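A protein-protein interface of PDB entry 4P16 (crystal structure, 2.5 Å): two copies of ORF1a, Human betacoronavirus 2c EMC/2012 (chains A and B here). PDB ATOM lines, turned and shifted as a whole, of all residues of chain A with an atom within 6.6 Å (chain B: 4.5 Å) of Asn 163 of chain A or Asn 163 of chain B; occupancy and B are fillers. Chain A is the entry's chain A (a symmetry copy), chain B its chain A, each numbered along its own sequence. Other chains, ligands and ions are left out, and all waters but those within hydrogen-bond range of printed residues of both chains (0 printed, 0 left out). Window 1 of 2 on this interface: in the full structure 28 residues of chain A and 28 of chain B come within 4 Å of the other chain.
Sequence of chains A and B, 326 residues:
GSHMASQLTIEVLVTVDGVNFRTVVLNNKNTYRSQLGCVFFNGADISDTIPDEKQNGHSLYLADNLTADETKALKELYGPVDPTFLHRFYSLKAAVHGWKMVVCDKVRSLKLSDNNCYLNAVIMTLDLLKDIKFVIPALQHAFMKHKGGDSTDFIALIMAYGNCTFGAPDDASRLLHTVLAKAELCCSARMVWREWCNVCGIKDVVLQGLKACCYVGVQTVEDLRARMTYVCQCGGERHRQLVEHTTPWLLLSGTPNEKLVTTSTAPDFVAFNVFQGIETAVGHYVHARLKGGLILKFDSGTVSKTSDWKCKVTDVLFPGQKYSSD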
ATOM      1  N   ASP A  82      -7.328   2.228  20.781  1.00  0.00           N
ATOM      2  CA  ASP A  82      -7.707   1.360  19.662  1.00  0.00           C
ATOM      3  C   ASP A  82      -6.868   0.062  19.747  1.00  0.00           C
ATOM      4  O   ASP A  82      -5.859   0.048  20.463  1.00  0.00           O
ATOM      5  CB  ASP A  82      -7.582   2.086  18.308  1.00  0.00           C
ATOM      6  CG  ASP A  82      -6.151   2.331  17.856  1.00  0.00           C
ATOM      7  OD1 ASP A  82      -5.581   1.441  17.162  1.00  0.00           O
ATOM      8  OD2 ASP A  82      -5.603   3.405  18.186  1.00  0.00           O
ATOM      9  N   THR A  84      -4.635  -1.281  17.941  1.00  0.00           N
ATOM     10  CA  THR A  84      -3.262  -1.250  17.401  1.00  0.00           C
ATOM     11  C   THR A  84      -2.338  -0.385  18.264  1.00  0.00           C
ATOM     12  O   THR A  84      -1.141  -0.232  17.942  1.00  0.00           O
ATOM     13  CB  THR A  84      -3.250  -0.799  15.909  1.00  0.00           C
ATOM     14  OG1 THR A  84      -3.403   0.619  15.817  1.00  0.00           O
ATOM     15  CG2 THR A  84      -4.307  -1.490  15.063  1.00  0.00           C
ATOM     16  N   ARG A  88       1.765   0.084  18.004  1.00  0.00           N
ATOM     17  CA  ARG A  88       2.301   1.389  17.573  1.00  0.00           C
ATOM     18  C   ARG A  88       3.170   2.015  18.668  1.00  0.00           C
ATOM     19  O   ARG A  88       4.294   2.414  18.375  1.00  0.00           O
ATOM     20  CB  ARG A  88       1.201   2.363  17.125  1.00  0.00           C
ATOM     21  CG  ARG A  88       0.478   1.921  15.850  1.00  0.00           C
ATOM     22  CD  ARG A  88      -0.593   2.912  15.412  1.00  0.00           C
ATOM     23  NE  ARG A  88      -1.702   3.014  16.375  1.00  0.00           N
ATOM     24  CZ  ARG A  88      -1.869   4.036  17.205  1.00  0.00           C
ATOM     25  NH1 ARG A  88      -1.010   5.043  17.206  1.00  0.00           N
ATOM     26  NH2 ARG A  88      -2.892   4.052  18.048  1.00  0.00           N
ATOM     27  N   ILE A 158       3.115  10.414  22.978  1.00  0.00           N
ATOM     28  CA  ILE A 158       2.509  11.582  22.331  1.00  0.00           C
ATOM     29  C   ILE A 158       2.284  11.197  20.889  1.00  0.00           C
ATOM     30  O   ILE A 158       1.178  11.308  20.398  1.00  0.00           O
ATOM     31  CB  ILE A 158       3.429  12.826  22.461  1.00  0.00           C
ATOM     32  CG1 ILE A 158       3.435  13.366  23.871  1.00  0.00           C
ATOM     33  CG2 ILE A 158       3.048  13.922  21.477  1.00  0.00           C
ATOM     34  CD1 ILE A 158       4.525  14.227  24.035  1.00  0.00           C
ATOM     35  N   MET A 159       3.313  10.671  20.239  1.00  0.00           N
ATOM     36  CA  MET A 159       3.228  10.183  18.866  1.00  0.00           C
ATOM     37  C   MET A 159       2.161   9.057  18.703  1.00  0.00           C
ATOM     38  O   MET A 159       1.503   8.992  17.669  1.00  0.00           O
ATOM     39  CB  MET A 159       4.604   9.672  18.408  1.00  0.00           C
ATOM     40  CG  MET A 159       5.622  10.749  18.260  1.00  0.00           C
ATOM     41  SD  MET A 159       7.157  10.009  17.690  1.00  0.00           S
ATOM     42  CE  MET A 159       6.860  10.020  15.912  1.00  0.00           C
ATOM     43  N   ALA A 160       2.003   8.186  19.720  1.00  0.00           N
ATOM     44  CA  ALA A 160       1.050   7.078  19.686  1.00  0.00           C
ATOM     45  C   ALA A 160      -0.382   7.601  19.796  1.00  0.00           C
ATOM     46  O   ALA A 160      -1.222   7.215  18.989  1.00  0.00           O
ATOM     47  CB  ALA A 160       1.355   6.082  20.798  1.00  0.00           C
ATOM     48  N   TYR A 161      -0.654   8.486  20.789  1.00  0.00           N
ATOM     49  CA  TYR A 161      -1.969   9.124  20.992  1.00  0.00           C
ATOM     50  C   TYR A 161      -2.326  10.090  19.851  1.00  0.00           C
ATOM     51  O   TYR A 161      -3.476  10.173  19.453  1.00  0.00           O
ATOM     52  CB  TYR A 161      -2.027   9.855  22.329  1.00  0.00           C
ATOM     53  CG  TYR A 161      -2.127   8.948  23.532  1.00  0.00           C
ATOM     54  CD1 TYR A 161      -3.302   8.255  23.814  1.00  0.00           C
ATOM     55  CD2 TYR A 161      -1.088   8.869  24.454  1.00  0.00           C
ATOM     56  CE1 TYR A 161      -3.400   7.423  24.927  1.00  0.00           C
ATOM     57  CE2 TYR A 161      -1.172   8.039  25.571  1.00  0.00           C
ATOM     58  CZ  TYR A 161      -2.340   7.337  25.818  1.00  0.00           C
ATOM     59  OH  TYR A 161      -2.435   6.545  26.930  1.00  0.00           O
ATOM     60  N   GLY A 162      -1.334  10.759  19.301  1.00  0.00           N
ATOM     61  CA  GLY A 162      -1.541  11.670  18.185  1.00  0.00           C
ATOM     62  C   GLY A 162      -1.627  11.046  16.800  1.00  0.00           C
ATOM     63  O   GLY A 162      -1.956  11.749  15.834  1.00  0.00           O
ATOM     64  N   ASN A 163      -1.354   9.729  16.690  1.00  0.00           N
ATOM     65  CA  ASN A 163      -1.361   8.948  15.445  1.00  0.00           C
ATOM     66  C   ASN A 163      -0.318   9.496  14.473  1.00  0.00           C
ATOM     67  O   ASN A 163      -0.581   9.670  13.289  1.00  0.00           O
ATOM     68  CB  ASN A 163      -2.775   8.836  14.813  1.00  0.00           C
ATOM     69  CG  ASN A 163      -3.784   8.115  15.681  1.00  0.00           C
ATOM     70  OD1 ASN A 163      -3.711   6.892  15.914  1.00  0.00           O
ATOM     71  ND2 ASN A 163      -4.752   8.866  16.173  1.00  0.00           N
ATOM     72  N   CYS A 164       0.871   9.772  15.016  1.00  0.00           N
ATOM     73  CA  CYS A 164       2.047  10.322  14.338  1.00  0.00           C
ATOM     74  C   CYS A 164       2.899   9.144  13.856  1.00  0.00           C
ATOM     75  O   CYS A 164       3.168   8.225  14.640  1.00  0.00           O
ATOM     76  CB  CYS A 164       2.837  11.226  15.288  1.00  0.00           C
ATOM     77  SG  CYS A 164       1.921  12.660  15.919  1.00  0.00           S
ATOM     78  N   THR A 165       3.345   9.176  12.591  1.00  0.00           N
ATOM     79  CA  THR A 165       4.170   8.105  12.025  1.00  0.00           C
ATOM     80  C   THR A 165       5.636   8.491  12.131  1.00  0.00           C
ATOM     81  O   THR A 165       5.986   9.639  11.846  1.00  0.00           O
ATOM     82  CB  THR A 165       3.714   7.808  10.571  1.00  0.00           C
ATOM     83  OG1 THR A 165       2.442   7.165  10.609  1.00  0.00           O
ATOM     84  CG2 THR A 165       4.692   6.918   9.784  1.00  0.00           C
ATOM     85  N   ASP A 170       4.382  16.713  11.011  1.00  0.00           N
ATOM     86  CA  ASP A 170       3.053  16.877  11.593  1.00  0.00           C
ATOM     87  C   ASP A 170       2.752  18.318  12.051  1.00  0.00           C
ATOM     88  O   ASP A 170       3.551  19.221  11.799  1.00  0.00           O
ATOM     89  CB  ASP A 170       2.864  15.863  12.732  1.00  0.00           C
ATOM     90  CG  ASP A 170       1.505  15.192  12.788  1.00  0.00           C
ATOM     91  OD1 ASP A 170       0.464  15.929  12.748  1.00  0.00           O
ATOM     92  OD2 ASP A 170       1.466  13.934  12.907  1.00  0.00           O
ATOM     93  N   ARG A 174      -1.951  20.852  16.575  1.00  0.00           N
ATOM     94  CA  ARG A 174      -2.813  19.666  16.621  1.00  0.00           C
ATOM     95  C   ARG A 174      -2.428  18.796  17.788  1.00  0.00           C
ATOM     96  O   ARG A 174      -3.258  18.553  18.678  1.00  0.00           O
ATOM     97  CB  ARG A 174      -2.758  18.845  15.321  1.00  0.00           C
ATOM     98  CG  ARG A 174      -3.718  17.666  15.368  1.00  0.00           C
ATOM     99  CD  ARG A 174      -3.682  16.781  14.141  1.00  0.00           C
ATOM    100  NE  ARG A 174      -2.468  15.977  14.019  1.00  0.00           N
ATOM    101  CZ  ARG A 174      -2.213  14.854  14.697  1.00  0.00           C
ATOM    102  NH1 ARG A 174      -1.099  14.179  14.472  1.00  0.00           N
ATOM    103  NH2 ARG A 174      -3.074  14.402  15.604  1.00  0.00           N
ATOM    104  N   LEU A 175      -1.141  18.404  17.819  1.00  0.00           N
ATOM    105  CA  LEU A 175      -0.598  17.559  18.861  1.00  0.00           C
ATOM    106  C   LEU A 175      -0.652  18.160  20.246  1.00  0.00           C
ATOM    107  O   LEU A 175      -1.046  17.446  21.173  1.00  0.00           O
ATOM    108  CB  LEU A 175       0.810  17.097  18.531  1.00  0.00           C
ATOM    109  CG  LEU A 175       0.976  15.609  18.226  1.00  0.00           C
ATOM    110  CD1 LEU A 175       2.418  15.222  18.392  1.00  0.00           C
ATOM    111  CD2 LEU A 175       0.170  14.726  19.184  1.00  0.00           C
ATOM    112  N   THR A 178      -4.268  18.011  21.513  1.00  0.00           N
ATOM    113  CA  THR A 178      -4.604  16.599  21.665  1.00  0.00           C
ATOM    114  C   THR A 178      -4.045  16.105  23.000  1.00  0.00           C
ATOM    115  O   THR A 178      -4.772  15.447  23.763  1.00  0.00           O
ATOM    116  CB  THR A 178      -3.997  15.778  20.501  1.00  0.00           C
ATOM    117  OG1 THR A 178      -4.467  16.285  19.252  1.00  0.00           O
ATOM    118  CG2 THR A 178      -4.304  14.268  20.608  1.00  0.00           C
ATOM    119  N   ARG B  88      -9.008  20.757   9.535  1.00  0.00           N
ATOM    120  CA  ARG B  88      -8.513  19.538   8.867  1.00  0.00           C
ATOM    121  C   ARG B  88      -9.612  18.893   8.016  1.00  0.00           C
ATOM    122  O   ARG B  88      -9.365  18.610   6.847  1.00  0.00           O
ATOM    123  CB  ARG B  88      -7.917  18.522   9.852  1.00  0.00           C
ATOM    124  CG  ARG B  88      -6.635  19.012  10.530  1.00  0.00           C
ATOM    125  CD  ARG B  88      -6.049  17.980  11.486  1.00  0.00           C
ATOM    126  NE  ARG B  88      -6.924  17.711  12.639  1.00  0.00           N
ATOM    127  CZ  ARG B  88      -7.657  16.613  12.770  1.00  0.00           C
ATOM    128  NH1 ARG B  88      -7.637  15.680  11.831  1.00  0.00           N
ATOM    129  NH2 ARG B  88      -8.426  16.445  13.838  1.00  0.00           N
ATOM    130  N   MET B 159     -10.505  10.174   7.245  1.00  0.00           N
ATOM    131  CA  MET B 159      -9.171  10.767   7.287  1.00  0.00           C
ATOM    132  C   MET B 159      -9.026  11.816   8.433  1.00  0.00           C
ATOM    133  O   MET B 159      -7.958  11.915   9.030  1.00  0.00           O
ATOM    134  CB  MET B 159      -8.849  11.421   5.933  1.00  0.00           C
ATOM    135  CG  MET B 159      -8.686  10.444   4.822  1.00  0.00           C
ATOM    136  SD  MET B 159      -8.281  11.347   3.322  1.00  0.00           S
ATOM    137  CE  MET B 159      -6.491  11.461   3.508  1.00  0.00           C
ATOM    138  N   ALA B 160     -10.095  12.583   8.724  1.00  0.00           N
ATOM    139  CA  ALA B 160     -10.084  13.612   9.763  1.00  0.00           C
ATOM    140  C   ALA B 160     -10.056  12.971  11.150  1.00  0.00           C
ATOM    141  O   ALA B 160      -9.226  13.356  11.969  1.00  0.00           O
ATOM    142  CB  ALA B 160     -11.289  14.533   9.611  1.00  0.00           C
ATOM    143  N   TYR B 161     -10.956  11.987  11.407  1.00  0.00           N
ATOM    144  CA  TYR B 161     -11.019  11.233  12.674  1.00  0.00           C
ATOM    145  C   TYR B 161      -9.783  10.341  12.879  1.00  0.00           C
ATOM    146  O   TYR B 161      -9.304  10.202  13.992  1.00  0.00           O
ATOM    147  CB  TYR B 161     -12.286  10.391  12.752  1.00  0.00           C
ATOM    148  CG  TYR B 161     -13.548  11.183  13.000  1.00  0.00           C
ATOM    149  CD1 TYR B 161     -13.803  11.756  14.244  1.00  0.00           C
ATOM    150  CD2 TYR B 161     -14.542  11.266  12.030  1.00  0.00           C
ATOM    151  CE1 TYR B 161     -14.969  12.481  14.479  1.00  0.00           C
ATOM    152  CE2 TYR B 161     -15.712  11.990  12.250  1.00  0.00           C
ATOM    153  CZ  TYR B 161     -15.933  12.576  13.487  1.00  0.00           C
ATOM    154  OH  TYR B 161     -17.096  13.262  13.714  1.00  0.00           O
ATOM    155  N   GLY B 162      -9.251   9.801  11.803  1.00  0.00           N
ATOM    156  CA  GLY B 162      -8.055   8.972  11.865  1.00  0.00           C
ATOM    157  C   GLY B 162      -6.721   9.702  11.918  1.00  0.00           C
ATOM    158  O   GLY B 162      -5.683   9.059  12.128  1.00  0.00           O
ATOM    159  N   ASN B 163      -6.733  11.041  11.750  1.00  0.00           N
ATOM    160  CA  ASN B 163      -5.556  11.920  11.746  1.00  0.00           C
ATOM    161  C   ASN B 163      -4.617  11.539  10.604  1.00  0.00           C
ATOM    162  O   ASN B 163      -3.408  11.445  10.779  1.00  0.00           O
ATOM    163  CB  ASN B 163      -4.841  11.974  13.124  1.00  0.00           C
ATOM    164  CG  ASN B 163      -5.692  12.538  14.240  1.00  0.00           C
ATOM    165  OD1 ASN B 163      -6.026  13.739  14.285  1.00  0.00           O
ATOM    166  ND2 ASN B 163      -6.058  11.675  15.171  1.00  0.00           N
ATOM    167  N   CYS B 164      -5.215  11.313   9.431  1.00  0.00           N
ATOM    168  CA  CYS B 164      -4.577  10.916   8.175  1.00  0.00           C
ATOM    169  C   CYS B 164      -4.247  12.193   7.396  1.00  0.00           C
ATOM    170  O   CYS B 164      -5.118  13.061   7.254  1.00  0.00           O
ATOM    171  CB  CYS B 164      -5.504  10.000   7.370  1.00  0.00           C
ATOM    172  SG  CYS B 164      -5.957   8.451   8.200  1.00  0.00           S
ATOM    173  N   THR B 165      -3.017  12.302   6.873  1.00  0.00           N
ATOM    174  CA  THR B 165      -2.594  13.478   6.108  1.00  0.00           C
ATOM    175  C   THR B 165      -2.768  13.201   4.624  1.00  0.00           C
ATOM    176  O   THR B 165      -2.418  12.112   4.162  1.00  0.00           O
ATOM    177  CB  THR B 165      -1.140  13.859   6.498  1.00  0.00           C
ATOM    178  OG1 THR B 165      -1.143  14.395   7.819  1.00  0.00           O
ATOM    179  CG2 THR B 165      -0.494  14.886   5.552  1.00  0.00           C
ATOM    180  N   ARG B 174      -5.706  -0.046  11.405  1.00  0.00           N
ATOM    181  CA  ARG B 174      -5.787   1.061  12.365  1.00  0.00           C
ATOM    182  C   ARG B 174      -7.042   1.857  12.126  1.00  0.00           C
ATOM    183  O   ARG B 174      -7.890   1.959  13.026  1.00  0.00           O
ATOM    184  CB  ARG B 174      -4.562   1.989  12.300  1.00  0.00           C
ATOM    185  CG  ARG B 174      -4.637   3.081  13.357  1.00  0.00           C
ATOM    186  CD  ARG B 174      -3.488   4.066  13.320  1.00  0.00           C
ATOM    187  NE  ARG B 174      -3.512   4.970  12.173  1.00  0.00           N
ATOM    188  CZ  ARG B 174      -4.291   6.049  12.054  1.00  0.00           C
ATOM    189  NH1 ARG B 174      -4.196   6.826  10.989  1.00  0.00           N
ATOM    190  NH2 ARG B 174      -5.171   6.354  13.003  1.00  0.00           N
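The side-chain amide oxygen of Asn 163 of chain B is in hydrogen-bond range of the guanidinium group of Arg 174 of chain A (3.3 Å). ND2 of Asn 163 of chain B sits close to ND2 of Asn 163 of chain A (3.3 Å). The guanidinium group (NH2) of Arg 174 of chain B sits at hydrogen-bond distance from the side-chain amide oxygen (OD1) of Asn 163 of chain A (3.3 Å).
O of Arg 174 of chain A is in hydrogen-bond range of OG1 of Thr 178 of chain A (2.6 Å). The side-chain sulfur (SG) of Cys 164 of chain A lies within hydrogen-bond range of the guanidinium group (NH1) of Arg 174 of chain A (3.7 Å). The side-chain sulfur of Cys 164 of chain B sits at hydrogen-bond distance from the guanidinium group of Arg 174 of chain B, at 3.7 Å. The guanidinium group of Arg 88 of chain A is in salt-bridge range of the side-chain carboxylate of Asp 82 of chain A (2.8 Å). NH2 of Arg 174 of chain B lies within hydrogen-bond range of O of Gly 162 of chain B, at 2.9 Å. The guanidinium group (NH1) of Arg 88 of chain A sits at hydrogen-bond distance from the backbone carbonyl oxygen (O) of Ala 160 of chain A (2.8 Å).
Among the printed residues, pairs that only touch across the chains: Thr 84 of chain A with Arg 174 of chain B, Arg 88 of chain A with Arg 174 of chain B, Gly 162 of chain A with Asn 163 of chain B, Asn 163 of chain A with Gly 162 of chain B and Arg 174 of chain A with Arg 88 of chain B.
Asn 163 of chain A touches just these residues of chain B: Gly 162, Asn 163 and Arg 174. Of chain A, only Gly 162, Asn 163 and Arg 174 come within 4 Å of Asn 163 of chain B. Of the printed residues of chain A, Gly 162 of chain B touches Asn 163 (3.96 Å). Printed residues of chain A within 4 Å of Arg 174 of chain B: Thr 84, Arg 88 and Asn 163. Printed residues of chain B within 4 Å of Arg 88 of chain A: Arg 174 (3.7 Å). Thr 165 of chain B touches none of the printed residues of chain A. The nearest printed residue of chain B that does not touch Asn 163 of chain A is Tyr 161 of chain B (5.2 Å). The nearest residue of chain A that does not touch Asn 163 of chain B is Tyr 161 of chain A (5.2 Å).
Printed residues of chain A that touch a printed residue of chain B: Thr 84, Arg 88, Gly 162, Asn 163 and Arg 174. Among the printed residues, no Asp or Glu carboxylate lies within 4 Å of a Lys or Arg side-chain nitrogen of the other chain.
Arg 88 of chain A touches Arg 174 of chain B, and with the chains exchanged Arg 174 of chain A touches Arg 88 of chain B. Gly 162 of chain A touches Asn 163 of chain B, and with the chains exchanged Asn 163 of chain A touches Gly 162 of chain B. Asn 163 of chain B touches its own counterpart, Asn 163 of chain A. Asn 163 of chain A touches Arg 174 of chain B, and with the chains exchanged Arg 174 of chain A touches Asn 163 of chain B. 9 positions are printed for both chains. Of the 8 pairs that touch across the chains among the printed residues, 7 have their exchanged pair printed and touching as well.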
